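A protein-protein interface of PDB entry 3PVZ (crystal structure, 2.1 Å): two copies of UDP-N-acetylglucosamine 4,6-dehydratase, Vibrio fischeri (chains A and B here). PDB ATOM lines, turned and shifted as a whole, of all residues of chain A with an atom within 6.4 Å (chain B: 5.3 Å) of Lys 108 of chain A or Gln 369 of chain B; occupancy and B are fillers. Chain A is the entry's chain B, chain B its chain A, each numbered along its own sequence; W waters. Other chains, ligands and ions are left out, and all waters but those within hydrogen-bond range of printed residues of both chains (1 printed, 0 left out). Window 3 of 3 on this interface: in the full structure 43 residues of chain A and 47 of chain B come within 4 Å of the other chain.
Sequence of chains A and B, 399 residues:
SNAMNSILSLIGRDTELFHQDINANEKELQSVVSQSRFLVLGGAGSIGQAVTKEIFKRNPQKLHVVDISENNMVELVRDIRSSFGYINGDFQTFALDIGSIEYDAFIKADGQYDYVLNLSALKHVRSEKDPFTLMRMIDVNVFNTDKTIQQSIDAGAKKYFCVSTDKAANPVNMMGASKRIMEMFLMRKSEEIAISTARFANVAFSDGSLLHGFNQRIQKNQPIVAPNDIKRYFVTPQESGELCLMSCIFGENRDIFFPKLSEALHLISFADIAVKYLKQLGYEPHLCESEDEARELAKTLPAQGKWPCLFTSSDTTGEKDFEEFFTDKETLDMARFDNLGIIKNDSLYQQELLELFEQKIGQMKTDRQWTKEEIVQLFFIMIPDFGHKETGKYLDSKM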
ATOM      1  N   TYR A 103      13.956  12.482 -34.724  1.00  0.00           N
ATOM      2  CA  TYR A 103      13.776  11.299 -35.552  1.00  0.00           C
ATOM      3  C   TYR A 103      14.266  10.057 -34.851  1.00  0.00           C
ATOM      4  O   TYR A 103      13.658   9.002 -34.992  1.00  0.00           O
ATOM      5  CB  TYR A 103      14.520  11.407 -36.871  1.00  0.00           C
ATOM      6  CG  TYR A 103      14.304  10.227 -37.808  1.00  0.00           C
ATOM      7  CD1 TYR A 103      15.202   9.151 -37.849  1.00  0.00           C
ATOM      8  CD2 TYR A 103      13.201  10.170 -38.609  1.00  0.00           C
ATOM      9  CE1 TYR A 103      14.982   8.049 -38.700  1.00  0.00           C
ATOM     10  CE2 TYR A 103      12.986   9.088 -39.490  1.00  0.00           C
ATOM     11  CZ  TYR A 103      13.890   8.047 -39.537  1.00  0.00           C
ATOM     12  OH  TYR A 103      13.664   7.010 -40.397  1.00  0.00           O
ATOM     13  N   ASP A 104      15.366  10.157 -34.115  1.00  0.00           N
ATOM     14  CA  ASP A 104      15.875   8.965 -33.477  1.00  0.00           C
ATOM     15  C   ASP A 104      14.858   8.547 -32.419  1.00  0.00           C
ATOM     16  O   ASP A 104      14.544   7.357 -32.341  1.00  0.00           O
ATOM     17  CB  ASP A 104      17.249   9.164 -32.867  1.00  0.00           C
ATOM     18  CG  ASP A 104      18.367   9.245 -33.918  1.00  0.00           C
ATOM     19  OD1 ASP A 104      18.190   8.811 -35.072  1.00  0.00           O
ATOM     20  OD2 ASP A 104      19.456   9.750 -33.569  1.00  0.00           O
ATOM     21  N   ALA A 105      14.349   9.522 -31.636  1.00  0.00           N
ATOM     22  CA  ALA A 105      13.259   9.283 -30.668  1.00  0.00           C
ATOM     23  C   ALA A 105      12.042   8.632 -31.323  1.00  0.00           C
ATOM     24  O   ALA A 105      11.501   7.695 -30.789  1.00  0.00           O
ATOM     25  CB  ALA A 105      12.840  10.567 -29.984  1.00  0.00           C
ATOM     26  N   PHE A 106      11.633   9.155 -32.469  1.00  0.00           N
ATOM     27  CA  PHE A 106      10.533   8.604 -33.274  1.00  0.00           C
ATOM     28  C   PHE A 106      10.741   7.098 -33.514  1.00  0.00           C
ATOM     29  O   PHE A 106       9.879   6.273 -33.227  1.00  0.00           O
ATOM     30  CB  PHE A 106      10.396   9.414 -34.595  1.00  0.00           C
ATOM     31  CG  PHE A 106       9.583   8.746 -35.690  1.00  0.00           C
ATOM     32  CD1 PHE A 106       8.206   8.673 -35.621  1.00  0.00           C
ATOM     33  CD2 PHE A 106      10.191   8.284 -36.817  1.00  0.00           C
ATOM     34  CE1 PHE A 106       7.470   8.087 -36.634  1.00  0.00           C
ATOM     35  CE2 PHE A 106       9.472   7.720 -37.849  1.00  0.00           C
ATOM     36  CZ  PHE A 106       8.104   7.619 -37.755  1.00  0.00           C
ATOM     37  N   ILE A 107      11.912   6.745 -33.991  1.00  0.00           N
ATOM     38  CA  ILE A 107      12.231   5.372 -34.284  1.00  0.00           C
ATOM     39  C   ILE A 107      12.299   4.527 -33.007  1.00  0.00           C
ATOM     40  O   ILE A 107      11.815   3.397 -32.973  1.00  0.00           O
ATOM     41  CB  ILE A 107      13.565   5.266 -35.035  1.00  0.00           C
ATOM     42  CG1 ILE A 107      13.451   5.843 -36.454  1.00  0.00           C
ATOM     43  CG2 ILE A 107      14.008   3.811 -35.112  1.00  0.00           C
ATOM     44  CD1 ILE A 107      12.540   5.037 -37.412  1.00  0.00           C
ATOM     45  N   LYS A 108      12.899   5.069 -31.963  1.00  0.00           N
ATOM     46  CA  LYS A 108      13.024   4.306 -30.740  1.00  0.00           C
ATOM     47  C   LYS A 108      11.642   4.005 -30.185  1.00  0.00           C
ATOM     48  O   LYS A 108      11.435   2.935 -29.659  1.00  0.00           O
ATOM     49  CB  LYS A 108      13.868   5.036 -29.710  1.00  0.00           C
ATOM     50  CG  LYS A 108      14.088   4.246 -28.458  1.00  0.00           C
ATOM     51  CD  LYS A 108      14.774   5.050 -27.378  1.00  0.00           C
ATOM     52  CE  LYS A 108      14.870   4.266 -26.085  1.00  0.00           C
ATOM     53  NZ  LYS A 108      14.976   5.182 -24.906  1.00  0.00           N
ATOM     54  N   ALA A 109      10.692   4.925 -30.331  1.00  0.00           N
ATOM     55  CA  ALA A 109       9.318   4.721 -29.836  1.00  0.00           C
ATOM     56  C   ALA A 109       8.504   3.688 -30.642  1.00  0.00           C
ATOM     57  O   ALA A 109       7.518   3.127 -30.119  1.00  0.00           O
ATOM     58  CB  ALA A 109       8.556   6.058 -29.742  1.00  0.00           C
ATOM     59  N   ASP A 110       8.908   3.416 -31.882  1.00  0.00           N
ATOM     60  CA  ASP A 110       8.154   2.492 -32.725  1.00  0.00           C
ATOM     61  C   ASP A 110       9.101   1.706 -33.616  1.00  0.00           C
ATOM     62  O   ASP A 110       9.515   0.597 -33.278  1.00  0.00           O
ATOM     63  CB  ASP A 110       7.110   3.287 -33.534  1.00  0.00           C
ATOM     64  CG  ASP A 110       6.292   2.427 -34.486  1.00  0.00           C
ATOM     65  OD1 ASP A 110       6.458   1.189 -34.541  1.00  0.00           O
ATOM     66  OD2 ASP A 110       5.460   3.005 -35.198  1.00  0.00           O
ATOM     67  N   GLY A 111       9.426   2.286 -34.762  1.00  0.00           N
ATOM     68  CA  GLY A 111      10.388   1.711 -35.703  1.00  0.00           C
ATOM     69  C   GLY A 111       9.944   0.439 -36.400  1.00  0.00           C
ATOM     70  O   GLY A 111      10.719  -0.149 -37.129  1.00  0.00           O
ATOM     71  N   MET B 364      14.931  15.546 -21.628  1.00  0.00           N
ATOM     72  CA  MET B 364      14.119  14.744 -22.511  1.00  0.00           C
ATOM     73  C   MET B 364      14.987  14.256 -23.677  1.00  0.00           C
ATOM     74  O   MET B 364      14.911  13.111 -24.073  1.00  0.00           O
ATOM     75  CB  MET B 364      12.928  15.539 -23.029  1.00  0.00           C
ATOM     76  CG  MET B 364      11.831  15.769 -22.005  1.00  0.00           C
ATOM     77  SD  MET B 364      10.386  16.833 -22.776  1.00  0.00           S
ATOM     78  CE  MET B 364      10.207  18.149 -21.326  1.00  0.00           C
ATOM     79  N   ASP B 367      17.355  11.445 -22.503  1.00  0.00           N
ATOM     80  CA  ASP B 367      16.623  10.213 -22.291  1.00  0.00           C
ATOM     81  C   ASP B 367      16.202   9.531 -23.601  1.00  0.00           C
ATOM     82  O   ASP B 367      15.842   8.349 -23.605  1.00  0.00           O
ATOM     83  CB  ASP B 367      15.398  10.476 -21.400  1.00  0.00           C
ATOM     84  CG  ASP B 367      15.772  11.073 -20.034  1.00  0.00           C
ATOM     85  OD1 ASP B 367      16.960  11.010 -19.652  1.00  0.00           O
ATOM     86  OD2 ASP B 367      14.881  11.622 -19.350  1.00  0.00           O
ATOM     87  N   ARG B 368      16.267  10.274 -24.700  1.00  0.00           N
ATOM     88  CA  ARG B 368      15.903   9.806 -26.040  1.00  0.00           C
ATOM     89  C   ARG B 368      14.448   9.417 -26.100  1.00  0.00           C
ATOM     90  O   ARG B 368      14.033   8.699 -27.009  1.00  0.00           O
ATOM     91  CB  ARG B 368      16.768   8.629 -26.543  1.00  0.00           C
ATOM     92  CG  ARG B 368      18.292   8.710 -26.359  1.00  0.00           C
ATOM     93  CD  ARG B 368      18.902  10.002 -26.783  1.00  0.00           C
ATOM     94  NE  ARG B 368      19.655   9.950 -28.042  1.00  0.00           N
ATOM     95  CZ  ARG B 368      20.401  10.967 -28.489  1.00  0.00           C
ATOM     96  NH1 ARG B 368      20.505  12.077 -27.756  1.00  0.00           N
ATOM     97  NH2 ARG B 368      21.068  10.878 -29.647  1.00  0.00           N
ATOM     98  N   GLN B 369      13.672   9.897 -25.138  1.00  0.00           N
ATOM     99  CA  GLN B 369      12.247   9.561 -25.043  1.00  0.00           C
ATOM    100  C   GLN B 369      11.523  10.617 -24.226  1.00  0.00           C
ATOM    101  O   GLN B 369      12.064  11.115 -23.232  1.00  0.00           O
ATOM    102  CB  GLN B 369      12.042   8.157 -24.425  1.00  0.00           C
ATOM    103  CG  GLN B 369      11.948   8.096 -22.876  1.00  0.00           C
ATOM    104  CD  GLN B 369      12.502   6.789 -22.270  1.00  0.00           C
ATOM    105  OE1 GLN B 369      12.248   5.681 -22.769  1.00  0.00           O
ATOM    106  NE2 GLN B 369      13.265   6.927 -21.182  1.00  0.00           N
ATOM    107  N   TRP B 370      10.302  10.918 -24.637  1.00  0.00           N
ATOM    108  CA  TRP B 370       9.467  11.885 -23.990  1.00  0.00           C
ATOM    109  C   TRP B 370       8.046  11.758 -24.560  1.00  0.00           C
ATOM    110  O   TRP B 370       7.837  11.198 -25.646  1.00  0.00           O
ATOM    111  CB  TRP B 370      10.025  13.297 -24.193  1.00  0.00           C
ATOM    112  CG  TRP B 370      10.081  13.755 -25.602  1.00  0.00           C
ATOM    113  CD1 TRP B 370       9.105  14.370 -26.277  1.00  0.00           C
ATOM    114  CD2 TRP B 370      11.200  13.671 -26.502  1.00  0.00           C
ATOM    115  NE1 TRP B 370       9.514  14.673 -27.547  1.00  0.00           N
ATOM    116  CE2 TRP B 370      10.802  14.255 -27.710  1.00  0.00           C
ATOM    117  CE3 TRP B 370      12.497  13.176 -26.390  1.00  0.00           C
ATOM    118  CZ2 TRP B 370      11.640  14.340 -28.820  1.00  0.00           C
ATOM    119  CZ3 TRP B 370      13.329  13.255 -27.481  1.00  0.00           C
ATOM    120  CH2 TRP B 370      12.897  13.835 -28.692  1.00  0.00           C
ATOM    121  N   THR B 371       7.079  12.276 -23.812  1.00  0.00           N
ATOM    122  CA  THR B 371       5.678  12.197 -24.177  1.00  0.00           C
ATOM    123  C   THR B 371       5.219  13.592 -24.531  1.00  0.00           C
ATOM    124  O   THR B 371       5.797  14.571 -24.056  1.00  0.00           O
ATOM    125  CB  THR B 371       4.849  11.733 -22.995  1.00  0.00           C
ATOM    126  OG1 THR B 371       5.061  12.639 -21.914  1.00  0.00           O
ATOM    127  CG2 THR B 371       5.234  10.282 -22.546  1.00  0.00           C
ATOM    128  N   GLU B 374       4.240  15.398 -21.274  1.00  0.00           N
ATOM    129  CA  GLU B 374       5.377  15.937 -20.539  1.00  0.00           C
ATOM    130  C   GLU B 374       5.721  17.364 -21.005  1.00  0.00           C
ATOM    131  O   GLU B 374       6.031  18.238 -20.189  1.00  0.00           O
ATOM    132  CB  GLU B 374       6.578  15.040 -20.784  1.00  0.00           C
ATOM    133  CG  GLU B 374       7.584  14.978 -19.674  1.00  0.00           C
ATOM    134  CD  GLU B 374       8.753  14.103 -20.040  1.00  0.00           C
ATOM    135  OE1 GLU B 374       8.635  13.329 -21.025  1.00  0.00           O
ATOM    136  OE2 GLU B 374       9.799  14.214 -19.356  1.00  0.00           O
HETATM  137  O   HOH W   1      11.751   7.652 -27.738  1.00  0.00           O
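Among the printed residues, merely in contact across the chains: Lys 108 of chain A with Gln 369 of chain B, Ala 105 of chain A with Trp 370 of chain B, Lys 108 of chain A with Asp 367 of chain B, Ala 105 of chain A with Arg 368 of chain B and Lys 108 of chain A with Arg 368 of chain B.
Of the printed residues of chain B, Ala 105 of chain A touches Arg 368 and Trp 370. Printed residues of chain B within 4 Å of Lys 108 of chain A: Asp 367 (3.5 Å), Arg 368 (3.7 Å) and Gln 369 (3.5 Å). Asp 110 of chain A touches none of the printed residues of chain B. Of the printed residues of chain A, Asp 367 of chain B touches Lys 108 (3.5 Å). Of the printed residues of chain A, Arg 368 of chain B touches Ala 105 (3.7 Å) and Lys 108 (3.7 Å). Of the printed residues of chain A, Gln 369 of chain B touches Lys 108 (3.5 Å). Printed residues of chain A within 4 Å of Trp 370 of chain B: Ala 105 (3.5 Å). The nearest printed residue of chain B that does not touch Lys 108 of chain A is Trp 370 of chain B (7.4 Å). The nearest printed residue of chain A that does not touch Asp 367 of chain B is Ala 105 of chain A (7.3 Å).
Of the 9 printed residues of chain A, 2 touch a printed residue of chain B. Hydrophobic or aromatic side chains of chain A that line the printed part of chain B: Ala 105. Of the 7 printed residues of chain B, 4 touch a printed residue of chain A. Printed residues of chain B that touch a printed residue of chain A: Asp 367, Arg 368, Gln 369 and Trp 370. Among the printed residues, 5 pairs touch across the chains.
No position is printed for both chains. Of the 5 pairs that touch across the chains among the printed residues, none has its exchanged pair printed and touching as well.
Water W1 bridges the backbone carbonyl oxygen (O) of Arg 368 of chain B (2.6 Å) and the backbone carbonyl oxygen (O) of Ala 105 of chain A (3.1 Å).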
